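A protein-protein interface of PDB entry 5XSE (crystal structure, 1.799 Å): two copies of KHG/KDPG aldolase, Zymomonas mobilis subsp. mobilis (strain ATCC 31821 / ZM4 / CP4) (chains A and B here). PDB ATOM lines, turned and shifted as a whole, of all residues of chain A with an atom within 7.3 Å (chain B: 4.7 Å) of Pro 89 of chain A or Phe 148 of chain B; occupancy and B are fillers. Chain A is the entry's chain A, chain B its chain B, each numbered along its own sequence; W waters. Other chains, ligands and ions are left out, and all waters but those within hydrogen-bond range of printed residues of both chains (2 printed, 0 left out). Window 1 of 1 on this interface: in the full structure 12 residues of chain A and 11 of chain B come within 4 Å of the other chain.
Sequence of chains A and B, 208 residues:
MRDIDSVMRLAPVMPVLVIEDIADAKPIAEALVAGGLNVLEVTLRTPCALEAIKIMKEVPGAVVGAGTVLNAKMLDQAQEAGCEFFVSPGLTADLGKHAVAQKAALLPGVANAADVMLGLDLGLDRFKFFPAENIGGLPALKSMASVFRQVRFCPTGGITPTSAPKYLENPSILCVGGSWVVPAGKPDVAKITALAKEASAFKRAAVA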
ATOM      1  N   GLU A  41      22.249   0.213   3.768  1.00  0.00           N
ATOM      2  CA  GLU A  41      22.988   0.676   2.594  1.00  0.00           C
ATOM      3  C   GLU A  41      22.926   2.204   2.523  1.00  0.00           C
ATOM      4  O   GLU A  41      21.870   2.777   2.237  1.00  0.00           O
ATOM      5  CB  GLU A  41      22.433   0.054   1.315  1.00  0.00           C
ATOM      6  CG  GLU A  41      23.098   0.601   0.069  1.00  0.00           C
ATOM      7  CD  GLU A  41      22.330   0.278  -1.193  1.00  0.00           C
ATOM      8  OE1 GLU A  41      21.528  -0.678  -1.165  1.00  0.00           O
ATOM      9  OE2 GLU A  41      22.531   0.986  -2.208  1.00  0.00           O
ATOM     10  N   ARG A  45      25.525   9.221  -2.660  1.00  0.00           N
ATOM     11  CA  ARG A  45      24.911  10.235  -3.505  1.00  0.00           C
ATOM     12  C   ARG A  45      24.912  11.628  -2.894  1.00  0.00           C
ATOM     13  O   ARG A  45      24.476  12.577  -3.559  1.00  0.00           O
ATOM     14  CB  ARG A  45      23.465   9.838  -3.842  1.00  0.00           C
ATOM     15  CG  ARG A  45      23.357   8.491  -4.522  1.00  0.00           C
ATOM     16  CD  ARG A  45      21.902   8.163  -4.787  1.00  0.00           C
ATOM     17  NE  ARG A  45      21.727   6.771  -5.162  1.00  0.00           N
ATOM     18  CZ  ARG A  45      20.538   6.214  -5.369  1.00  0.00           C
ATOM     19  NH1 ARG A  45      19.438   6.943  -5.222  1.00  0.00           N
ATOM     20  NH2 ARG A  45      20.449   4.938  -5.714  1.00  0.00           N
ATOM     21  N   GLY A  67      26.251   2.166  -0.851  1.00  0.00           N
ATOM     22  CA  GLY A  67      25.603   2.013  -2.134  1.00  0.00           C
ATOM     23  C   GLY A  67      26.095   3.056  -3.131  1.00  0.00           C
ATOM     24  O   GLY A  67      26.813   3.996  -2.787  1.00  0.00           O
ATOM     25  N   THR A  68      25.673   2.878  -4.386  1.00  0.00           N
ATOM     26  CA  THR A  68      26.086   3.736  -5.502  1.00  0.00           C
ATOM     27  C   THR A  68      27.611   3.826  -5.574  1.00  0.00           C
ATOM     28  O   THR A  68      28.189   4.885  -5.827  1.00  0.00           O
ATOM     29  CB  THR A  68      25.459   5.136  -5.415  1.00  0.00           C
ATOM     30  OG1 THR A  68      24.135   5.039  -4.882  1.00  0.00           O
ATOM     31  CG2 THR A  68      25.367   5.767  -6.812  1.00  0.00           C
ATOM     32  N   VAL A  69      28.269   2.701  -5.322  1.00  0.00           N
ATOM     33  CA  VAL A  69      29.712   2.618  -5.493  1.00  0.00           C
ATOM     34  C   VAL A  69      29.993   2.539  -6.985  1.00  0.00           C
ATOM     35  O   VAL A  69      29.506   1.632  -7.668  1.00  0.00           O
ATOM     36  CB  VAL A  69      30.289   1.408  -4.747  1.00  0.00           C
ATOM     37  CG1 VAL A  69      31.781   1.260  -5.044  1.00  0.00           C
ATOM     38  CG2 VAL A  69      30.049   1.570  -3.251  1.00  0.00           C
ATOM     39  N   LEU A  70      30.775   3.488  -7.495  1.00  0.00           N
ATOM     40  CA  LEU A  70      30.923   3.632  -8.934  1.00  0.00           C
ATOM     41  C   LEU A  70      32.241   3.100  -9.479  1.00  0.00           C
ATOM     42  O   LEU A  70      32.343   2.887 -10.691  1.00  0.00           O
ATOM     43  CB  LEU A  70      30.766   5.105  -9.337  1.00  0.00           C
ATOM     44  CG  LEU A  70      29.456   5.766  -8.910  1.00  0.00           C
ATOM     45  CD1 LEU A  70      29.438   7.238  -9.305  1.00  0.00           C
ATOM     46  CD2 LEU A  70      28.274   5.037  -9.525  1.00  0.00           C
ATOM     47  N   ASN A  71      33.242   2.877  -8.635  1.00  0.00           N
ATOM     48  CA  ASN A  71      34.555   2.492  -9.134  1.00  0.00           C
ATOM     49  C   ASN A  71      35.385   1.955  -7.978  1.00  0.00           C
ATOM     50  O   ASN A  71      34.971   2.000  -6.815  1.00  0.00           O
ATOM     51  CB  ASN A  71      35.263   3.666  -9.819  1.00  0.00           C
ATOM     52  CG  ASN A  71      35.442   4.846  -8.902  1.00  0.00           C
ATOM     53  OD1 ASN A  71      36.188   4.777  -7.929  1.00  0.00           O
ATOM     54  ND2 ASN A  71      34.776   5.953  -9.220  1.00  0.00           N
ATOM     55  N   VAL A  87      27.384  -1.866  -2.733  1.00  0.00           N
ATOM     56  CA  VAL A  87      26.353  -2.029  -3.749  1.00  0.00           C
ATOM     57  C   VAL A  87      26.663  -1.077  -4.891  1.00  0.00           C
ATOM     58  O   VAL A  87      27.001   0.090  -4.661  1.00  0.00           O
ATOM     59  CB  VAL A  87      24.938  -1.751  -3.187  1.00  0.00           C
ATOM     60  CG1 VAL A  87      23.870  -2.187  -4.188  1.00  0.00           C
ATOM     61  CG2 VAL A  87      24.749  -2.437  -1.845  1.00  0.00           C
ATOM     62  N   SER A  88      26.546  -1.566  -6.122  1.00  0.00           N
ATOM     63  CA  SER A  88      26.813  -0.707  -7.257  1.00  0.00           C
ATOM     64  C   SER A  88      25.645  -0.756  -8.233  1.00  0.00           C
ATOM     65  O   SER A  88      25.006  -1.803  -8.386  1.00  0.00           O
ATOM     66  CB  SER A  88      28.121  -1.117  -7.961  1.00  0.00           C
ATOM     67  OG  SER A  88      28.032  -2.412  -8.536  1.00  0.00           O
ATOM     68  N   PRO A  89      25.309   0.375  -8.864  1.00  0.00           N
ATOM     69  CA  PRO A  89      24.173   0.382  -9.803  1.00  0.00           C
ATOM     70  C   PRO A  89      24.360  -0.550 -10.986  1.00  0.00           C
ATOM     71  O   PRO A  89      23.374  -1.061 -11.528  1.00  0.00           O
ATOM     72  CB  PRO A  89      24.095   1.855 -10.235  1.00  0.00           C
ATOM     73  CG  PRO A  89      25.488   2.336 -10.138  1.00  0.00           C
ATOM     74  CD  PRO A  89      26.114   1.605  -8.970  1.00  0.00           C
ATOM     75  N   GLY A  90      25.604  -0.751 -11.416  1.00  0.00           N
ATOM     76  CA  GLY A  90      25.950  -1.605 -12.530  1.00  0.00           C
ATOM     77  C   GLY A  90      27.280  -2.256 -12.221  1.00  0.00           C
ATOM     78  O   GLY A  90      27.833  -2.089 -11.133  1.00  0.00           O
ATOM     79  N   LEU A  91      27.794  -3.009 -13.185  1.00  0.00           N
ATOM     80  CA  LEU A  91      29.043  -3.730 -13.000  1.00  0.00           C
ATOM     81  C   LEU A  91      30.010  -3.356 -14.112  1.00  0.00           C
ATOM     82  O   LEU A  91      29.679  -3.482 -15.295  1.00  0.00           O
ATOM     83  CB  LEU A  91      28.814  -5.248 -12.991  1.00  0.00           C
ATOM     84  CG  LEU A  91      30.079  -6.095 -12.759  1.00  0.00           C
ATOM     85  CD1 LEU A  91      30.672  -5.828 -11.384  1.00  0.00           C
ATOM     86  CD2 LEU A  91      29.822  -7.572 -12.928  1.00  0.00           C
ATOM     87  N   LEU A  95      35.653  -2.671 -11.571  1.00  0.00           N
ATOM     88  CA  LEU A  95      35.092  -2.655 -10.226  1.00  0.00           C
ATOM     89  C   LEU A  95      34.979  -4.065  -9.663  1.00  0.00           C
ATOM     90  O   LEU A  95      35.376  -4.320  -8.521  1.00  0.00           O
ATOM     91  CB  LEU A  95      33.726  -1.968 -10.232  1.00  0.00           C
ATOM     92  CG  LEU A  95      32.985  -2.014  -8.901  1.00  0.00           C
ATOM     93  CD1 LEU A  95      33.771  -1.271  -7.847  1.00  0.00           C
ATOM     94  CD2 LEU A  95      31.574  -1.447  -9.037  1.00  0.00           C
ATOM     95  N   LEU A 107      27.630  -6.303  -4.176  1.00  0.00           N
ATOM     96  CA  LEU A 107      26.346  -6.644  -4.784  1.00  0.00           C
ATOM     97  C   LEU A 107      26.179  -5.702  -5.967  1.00  0.00           C
ATOM     98  O   LEU A 107      25.654  -4.590  -5.814  1.00  0.00           O
ATOM     99  CB  LEU A 107      25.200  -6.487  -3.784  1.00  0.00           C
ATOM    100  CG  LEU A 107      23.791  -6.818  -4.282  1.00  0.00           C
ATOM    101  CD1 LEU A 107      23.671  -8.293  -4.642  1.00  0.00           C
ATOM    102  CD2 LEU A 107      22.732  -6.411  -3.246  1.00  0.00           C
ATOM    103  N   PRO A 108      26.625  -6.093  -7.158  1.00  0.00           N
ATOM    104  CA  PRO A 108      26.517  -5.212  -8.322  1.00  0.00           C
ATOM    105  C   PRO A 108      25.178  -5.327  -9.031  1.00  0.00           C
ATOM    106  O   PRO A 108      24.560  -6.393  -9.096  1.00  0.00           O
ATOM    107  CB  PRO A 108      27.656  -5.704  -9.228  1.00  0.00           C
ATOM    108  CG  PRO A 108      27.812  -7.156  -8.875  1.00  0.00           C
ATOM    109  CD  PRO A 108      27.283  -7.371  -7.480  1.00  0.00           C
ATOM    110  N   GLY A 109      24.743  -4.195  -9.582  1.00  0.00           N
ATOM    111  CA  GLY A 109      23.521  -4.187 -10.357  1.00  0.00           C
ATOM    112  C   GLY A 109      23.697  -4.853 -11.706  1.00  0.00           C
ATOM    113  O   GLY A 109      24.745  -4.750 -12.350  1.00  0.00           O
ATOM    114  N   VAL A 110      22.635  -5.524 -12.147  1.00  0.00           N
ATOM    115  CA  VAL A 110      22.539  -6.104 -13.480  1.00  0.00           C
ATOM    116  C   VAL A 110      21.187  -5.735 -14.079  1.00  0.00           C
ATOM    117  O   VAL A 110      20.182  -5.610 -13.370  1.00  0.00           O
ATOM    118  CB  VAL A 110      22.720  -7.645 -13.461  1.00  0.00           C
ATOM    119  CG1 VAL A 110      24.101  -8.020 -12.944  1.00  0.00           C
ATOM    120  CG2 VAL A 110      21.629  -8.340 -12.623  1.00  0.00           C
ATOM    121  N   ALA A 111      21.171  -5.558 -15.399  1.00  0.00           N
ATOM    122  CA  ALA A 111      19.934  -5.328 -16.141  1.00  0.00           C
ATOM    123  C   ALA A 111      19.760  -6.255 -17.339  1.00  0.00           C
ATOM    124  O   ALA A 111      18.666  -6.283 -17.919  1.00  0.00           O
ATOM    125  CB  ALA A 111      19.861  -3.873 -16.633  1.00  0.00           C
ATOM    126  N   ASP A 115      25.557  -8.398 -18.400  1.00  0.00           N
ATOM    127  CA  ASP A 115      25.985  -7.995 -17.063  1.00  0.00           C
ATOM    128  C   ASP A 115      26.237  -9.215 -16.190  1.00  0.00           C
ATOM    129  O   ASP A 115      27.277  -9.325 -15.536  1.00  0.00           O
ATOM    130  CB  ASP A 115      24.927  -7.107 -16.402  1.00  0.00           C
ATOM    131  CG  ASP A 115      24.698  -5.798 -17.140  1.00  0.00           C
ATOM    132  OD1 ASP A 115      25.640  -5.307 -17.797  1.00  0.00           O
ATOM    133  OD2 ASP A 115      23.574  -5.254 -17.024  1.00  0.00           O
ATOM    134  N   LYS A 128      22.059  -7.462  -7.724  1.00  0.00           N
ATOM    135  CA  LYS A 128      20.777  -6.797  -7.608  1.00  0.00           C
ATOM    136  C   LYS A 128      20.199  -6.552  -9.002  1.00  0.00           C
ATOM    137  O   LYS A 128      20.911  -6.173  -9.935  1.00  0.00           O
ATOM    138  CB  LYS A 128      20.876  -5.502  -6.783  1.00  0.00           C
ATOM    139  CG  LYS A 128      21.471  -4.290  -7.426  1.00  0.00           C
ATOM    140  CD  LYS A 128      21.125  -3.039  -6.585  1.00  0.00           C
ATOM    141  CE  LYS A 128      21.875  -1.805  -7.103  1.00  0.00           C
ATOM    142  NZ  LYS A 128      21.538  -0.545  -6.355  1.00  0.00           N
ATOM    143  N   PHE A 129      18.907  -6.842  -9.143  1.00  0.00           N
ATOM    144  CA  PHE A 129      18.162  -6.639 -10.382  1.00  0.00           C
ATOM    145  C   PHE A 129      17.674  -5.196 -10.341  1.00  0.00           C
ATOM    146  O   PHE A 129      16.735  -4.871  -9.612  1.00  0.00           O
ATOM    147  CB  PHE A 129      17.024  -7.651 -10.478  1.00  0.00           C
ATOM    148  CG  PHE A 129      16.256  -7.613 -11.779  1.00  0.00           C
ATOM    149  CD1 PHE A 129      16.788  -8.179 -12.935  1.00  0.00           C
ATOM    150  CD2 PHE A 129      14.983  -7.057 -11.833  1.00  0.00           C
ATOM    151  CE1 PHE A 129      16.065  -8.174 -14.127  1.00  0.00           C
ATOM    152  CE2 PHE A 129      14.263  -7.043 -13.017  1.00  0.00           C
ATOM    153  CZ  PHE A 129      14.806  -7.600 -14.166  1.00  0.00           C
ATOM    154  N   PHE A 130      18.345  -4.318 -11.097  1.00  0.00           N
ATOM    155  CA  PHE A 130      18.226  -2.873 -10.887  1.00  0.00           C
ATOM    156  C   PHE A 130      18.349  -2.099 -12.189  1.00  0.00           C
ATOM    157  O   PHE A 130      19.263  -2.380 -12.979  1.00  0.00           O
ATOM    158  CB  PHE A 130      19.317  -2.415  -9.908  1.00  0.00           C
ATOM    159  CG  PHE A 130      19.389  -0.929  -9.706  1.00  0.00           C
ATOM    160  CD1 PHE A 130      18.594  -0.311  -8.760  1.00  0.00           C
ATOM    161  CD2 PHE A 130      20.282  -0.153 -10.443  1.00  0.00           C
ATOM    162  CE1 PHE A 130      18.667   1.061  -8.559  1.00  0.00           C
ATOM    163  CE2 PHE A 130      20.364   1.205 -10.253  1.00  0.00           C
ATOM    164  CZ  PHE A 130      19.553   1.819  -9.305  1.00  0.00           C
ATOM    165  N   PRO A 131      17.488  -1.095 -12.425  1.00  0.00           N
ATOM    166  CA  PRO A 131      16.335  -0.733 -11.587  1.00  0.00           C
ATOM    167  C   PRO A 131      15.084  -1.510 -11.996  1.00  0.00           C
ATOM    168  O   PRO A 131      14.580  -1.317 -13.107  1.00  0.00           O
ATOM    169  CB  PRO A 131      16.170   0.767 -11.838  1.00  0.00           C
ATOM    170  CG  PRO A 131      16.735   0.995 -13.217  1.00  0.00           C
ATOM    171  CD  PRO A 131      17.750  -0.096 -13.482  1.00  0.00           C
ATOM    172  N   ALA B 113      22.981   1.357 -16.141  1.00  0.00           N
ATOM    173  CA  ALA B 113      23.957   1.945 -15.225  1.00  0.00           C
ATOM    174  C   ALA B 113      25.385   1.578 -15.607  1.00  0.00           C
ATOM    175  O   ALA B 113      26.301   2.396 -15.463  1.00  0.00           O
ATOM    176  CB  ALA B 113      23.660   1.508 -13.790  1.00  0.00           C
ATOM    177  N   VAL B 116      26.800   3.988 -18.044  1.00  0.00           N
ATOM    178  CA  VAL B 116      27.165   5.263 -17.433  1.00  0.00           C
ATOM    179  C   VAL B 116      28.439   5.118 -16.618  1.00  0.00           C
ATOM    180  O   VAL B 116      29.290   6.013 -16.607  1.00  0.00           O
ATOM    181  CB  VAL B 116      26.008   5.789 -16.567  1.00  0.00           C
ATOM    182  CG1 VAL B 116      26.386   7.102 -15.900  1.00  0.00           C
ATOM    183  CG2 VAL B 116      24.742   5.943 -17.394  1.00  0.00           C
ATOM    184  N   MET B 117      28.597   3.983 -15.937  1.00  0.00           N
ATOM    185  CA  MET B 117      29.805   3.756 -15.151  1.00  0.00           C
ATOM    186  C   MET B 117      31.036   3.671 -16.038  1.00  0.00           C
ATOM    187  O   MET B 117      32.099   4.201 -15.686  1.00  0.00           O
ATOM    188  CB  MET B 117      29.651   2.480 -14.326  1.00  0.00           C
ATOM    189  CG  MET B 117      28.664   2.618 -13.186  1.00  0.00           C
ATOM    190  SD  MET B 117      28.320   1.030 -12.400  1.00  0.00           S
ATOM    191  CE  MET B 117      29.938   0.584 -11.752  1.00  0.00           C
ATOM    192  N   LEU B 120      31.803   7.276 -16.938  1.00  0.00           N
ATOM    193  CA  LEU B 120      32.427   8.024 -15.849  1.00  0.00           C
ATOM    194  C   LEU B 120      33.876   7.592 -15.637  1.00  0.00           C
ATOM    195  O   LEU B 120      34.743   8.434 -15.363  1.00  0.00           O
ATOM    196  CB  LEU B 120      31.605   7.859 -14.566  1.00  0.00           C
ATOM    197  CG  LEU B 120      30.230   8.547 -14.555  1.00  0.00           C
ATOM    198  CD1 LEU B 120      29.395   8.087 -13.372  1.00  0.00           C
ATOM    199  CD2 LEU B 120      30.382  10.068 -14.527  1.00  0.00           C
ATOM    200  N   MET B 144      17.524   7.079 -13.253  1.00  0.00           N
ATOM    201  CA  MET B 144      18.949   7.054 -13.561  1.00  0.00           C
ATOM    202  C   MET B 144      19.612   8.385 -13.213  1.00  0.00           C
ATOM    203  O   MET B 144      20.748   8.415 -12.721  1.00  0.00           O
ATOM    204  CB  MET B 144      19.155   6.714 -15.036  1.00  0.00           C
ATOM    205  CG  MET B 144      20.590   6.890 -15.517  1.00  0.00           C
ATOM    206  SD  MET B 144      20.793   6.501 -17.260  1.00  0.00           S
ATOM    207  CE  MET B 144      20.457   4.733 -17.301  1.00  0.00           C
ATOM    208  N   ALA B 145      18.911   9.498 -13.444  1.00  0.00           N
ATOM    209  CA  ALA B 145      19.469  10.793 -13.071  1.00  0.00           C
ATOM    210  C   ALA B 145      19.580  10.929 -11.559  1.00  0.00           C
ATOM    211  O   ALA B 145      20.481  11.614 -11.061  1.00  0.00           O
ATOM    212  CB  ALA B 145      18.626  11.928 -13.655  1.00  0.00           C
ATOM    213  N   SER B 146      18.674  10.289 -10.821  1.00  0.00           N
ATOM    214  CA  SER B 146      18.746  10.321  -9.368  1.00  0.00           C
ATOM    215  C   SER B 146      19.962   9.563  -8.851  1.00  0.00           C
ATOM    216  O   SER B 146      20.517   9.924  -7.808  1.00  0.00           O
ATOM    217  CB  SER B 146      17.458   9.749  -8.782  1.00  0.00           C
ATOM    218  OG  SER B 146      17.467   9.847  -7.373  1.00  0.00           O
ATOM    219  N   VAL B 147      20.394   8.521  -9.566  1.00  0.00           N
ATOM    220  CA  VAL B 147      21.560   7.753  -9.142  1.00  0.00           C
ATOM    221  C   VAL B 147      22.851   8.489  -9.485  1.00  0.00           C
ATOM    222  O   VAL B 147      23.805   8.489  -8.700  1.00  0.00           O
ATOM    223  CB  VAL B 147      21.528   6.347  -9.771  1.00  0.00           C
ATOM    224  CG1 VAL B 147      22.803   5.584  -9.427  1.00  0.00           C
ATOM    225  CG2 VAL B 147      20.300   5.569  -9.299  1.00  0.00           C
ATOM    226  N   PHE B 148      22.914   9.113 -10.660  1.00  0.00           N
ATOM    227  CA  PHE B 148      24.132   9.759 -11.151  1.00  0.00           C
ATOM    228  C   PHE B 148      23.885  11.265 -11.181  1.00  0.00           C
ATOM    229  O   PHE B 148      23.615  11.853 -12.230  1.00  0.00           O
ATOM    230  CB  PHE B 148      24.525   9.224 -12.567  1.00  0.00           C
ATOM    231  CG  PHE B 148      24.728   7.737 -12.631  1.00  0.00           C
ATOM    232  CD1 PHE B 148      25.957   7.176 -12.301  1.00  0.00           C
ATOM    233  CD2 PHE B 148      23.707   6.905 -13.058  1.00  0.00           C
ATOM    234  CE1 PHE B 148      26.151   5.798 -12.373  1.00  0.00           C
ATOM    235  CE2 PHE B 148      23.891   5.529 -13.134  1.00  0.00           C
ATOM    236  CZ  PHE B 148      25.118   4.977 -12.793  1.00  0.00           C
ATOM    237  N   ARG B 149      23.996  11.898 -10.008  1.00  0.00           N
ATOM    238  CA  ARG B 149      23.630  13.307  -9.880  1.00  0.00           C
ATOM    239  C   ARG B 149      24.572  14.249 -10.621  1.00  0.00           C
ATOM    240  O   ARG B 149      24.167  15.372 -10.937  1.00  0.00           O
ATOM    241  CB  ARG B 149      23.556  13.700  -8.402  1.00  0.00           C
ATOM    242  CG  ARG B 149      22.225  13.342  -7.750  1.00  0.00           C
ATOM    243  CD  ARG B 149      22.415  12.326  -6.660  1.00  0.00           C
ATOM    244  NE  ARG B 149      21.166  11.965  -5.991  1.00  0.00           N
ATOM    245  CZ  ARG B 149      20.627  12.648  -4.985  1.00  0.00           C
ATOM    246  NH1 ARG B 149      21.205  13.757  -4.534  1.00  0.00           N
ATOM    247  NH2 ARG B 149      19.497  12.225  -4.432  1.00  0.00           N
ATOM    248  N   GLN B 150      25.804  13.834 -10.900  1.00  0.00           N
ATOM    249  CA  GLN B 150      26.753  14.675 -11.619  1.00  0.00           C
ATOM    250  C   GLN B 150      26.633  14.564 -13.138  1.00  0.00           C
ATOM    251  O   GLN B 150      27.359  15.255 -13.855  1.00  0.00           O
ATOM    252  CB  GLN B 150      28.185  14.343 -11.186  1.00  0.00           C
ATOM    253  CG  GLN B 150      28.343  14.045  -9.691  1.00  0.00           C
ATOM    254  CD  GLN B 150      27.833  15.159  -8.774  1.00  0.00           C
ATOM    255  OE1 GLN B 150      27.609  16.295  -9.204  1.00  0.00           O
ATOM    256  NE2 GLN B 150      27.656  14.830  -7.497  1.00  0.00           N
ATOM    257  N   VAL B 151      25.758  13.713 -13.642  1.00  0.00           N
ATOM    258  CA  VAL B 151      25.617  13.496 -15.077  1.00  0.00           C
ATOM    259  C   VAL B 151      24.454  14.324 -15.611  1.00  0.00           C
ATOM    260  O   VAL B 151      23.497  14.620 -14.894  1.00  0.00           O
ATOM    261  CB  VAL B 151      25.438  11.986 -15.345  1.00  0.00           C
ATOM    262  CG1 VAL B 151      25.126  11.711 -16.817  1.00  0.00           C
ATOM    263  CG2 VAL B 151      26.693  11.240 -14.911  1.00  0.00           C
HETATM  264  O   HOH W   1      18.910   9.900  -5.091  1.00  0.00           O
HETATM  265  O   HOH W   2      31.920   4.736 -12.878  1.00  0.00           O
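No position is printed for both chains. Of the 13 pairs that touch across the chains among the printed residues, none has its exchanged pair printed and touching as well.
Water W1 lies within hydrogen-bond range of the guanidinium group of Arg 149 of chain B (2.5 Å), the side-chain hydroxyl of Ser 146 of chain B (2.7 Å) and the guanidinium group of Arg 45 of chain A (3.0 Å). Water W2 lies within hydrogen-bond range of the backbone carbonyl oxygen of Met 117 of chain B (2.9 Å) and the backbone carbonyl oxygen of Leu 70 of chain A (2.9 Å).
Among the printed residues, merely in contact across the chains: Pro 89 of chain A with Ala 113 of chain B (3.4 Å), Leu 70 of chain A with Met 117 of chain B (3.5 Å), Arg 45 of chain A with Arg 149 of chain B (3.6 Å), Leu 70 of chain A with Phe 148 of chain B (3.6 Å), Arg 45 of chain A with Val 147 of chain B (3.6 Å), Thr 68 of chain A with Val 147 of chain B (3.7 Å), Arg 45 of chain A with Ser 146 of chain B (3.8 Å), Pro 89 of chain A with Phe 148 of chain B (3.8 Å), Leu 95 of chain A with Met 117 of chain B (3.8 Å), Gly 90 of chain A with Ala 113 of chain B (3.8 Å), Phe 130 of chain A with Val 147 of chain B (3.8 Å) and Pro 89 of chain A with Met 117 of chain B (3.9 Å).
Printed residues of chain B within 4 Å of Leu 70 of chain A: Met 117 (3.5 Å) and Phe 148 (3.6 Å). Of chain B, only Ala 113, Met 117 and Phe 148 come within 4 Å of Pro 89 of chain A. Of the printed residues of chain B, Gly 90 of chain A touches Ala 113 (3.8 Å) and Met 117 (3.4 Å). Printed residues of chain B within 4 Å of Leu 95 of chain A: Met 117. Printed residues of chain A within 4 Å of Ala 113 of chain B: Pro 89 (3.4 Å) and Gly 90 (3.8 Å). Ala 145 of chain B touches none of the printed residues of chain A. Of the printed residues of chain A, Arg 149 of chain B touches Arg 45 (3.6 Å). The nearest residue of chain A that does not touch Phe 148 of chain B is Thr 68 of chain A (5.6 Å).
Of the 23 printed residues of chain A, 7 touch a printed residue of chain B. Of the 12 printed residues of chain B, 6 touch a printed residue of chain A. Among the printed residues, no Asp or Glu carboxylate lies within 4 Å of a Lys or Arg side-chain nitrogen of the other chain.
N of Gly 90 of chain A lies within hydrogen-bond range of SD of Met 117 of chain B (3.4 Å).
OG1 of Thr 68 of chain A lies within hydrogen-bond range of NE of Arg 45 of chain A. N of Thr 68 of chain A sits at hydrogen-bond distance from O of Val 87 of chain A (3.1 Å). The side-chain hydroxyl (OG) of Ser 88 of chain A lies within hydrogen-bond range of the backbone carbonyl oxygen (O) of Gly 90 of chain A, 2.6 Å away. The backbone carbonyl oxygen (O) of Val 110 of chain A lies within hydrogen-bond range of the backbone NH (N) of Phe 130 of chain A (3.2 Å). The guanidinium group (NE) of Arg 149 of chain B is in hydrogen-bond range of the backbone carbonyl oxygen (O) of Ser 146 of chain B, 2.8 Å away.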
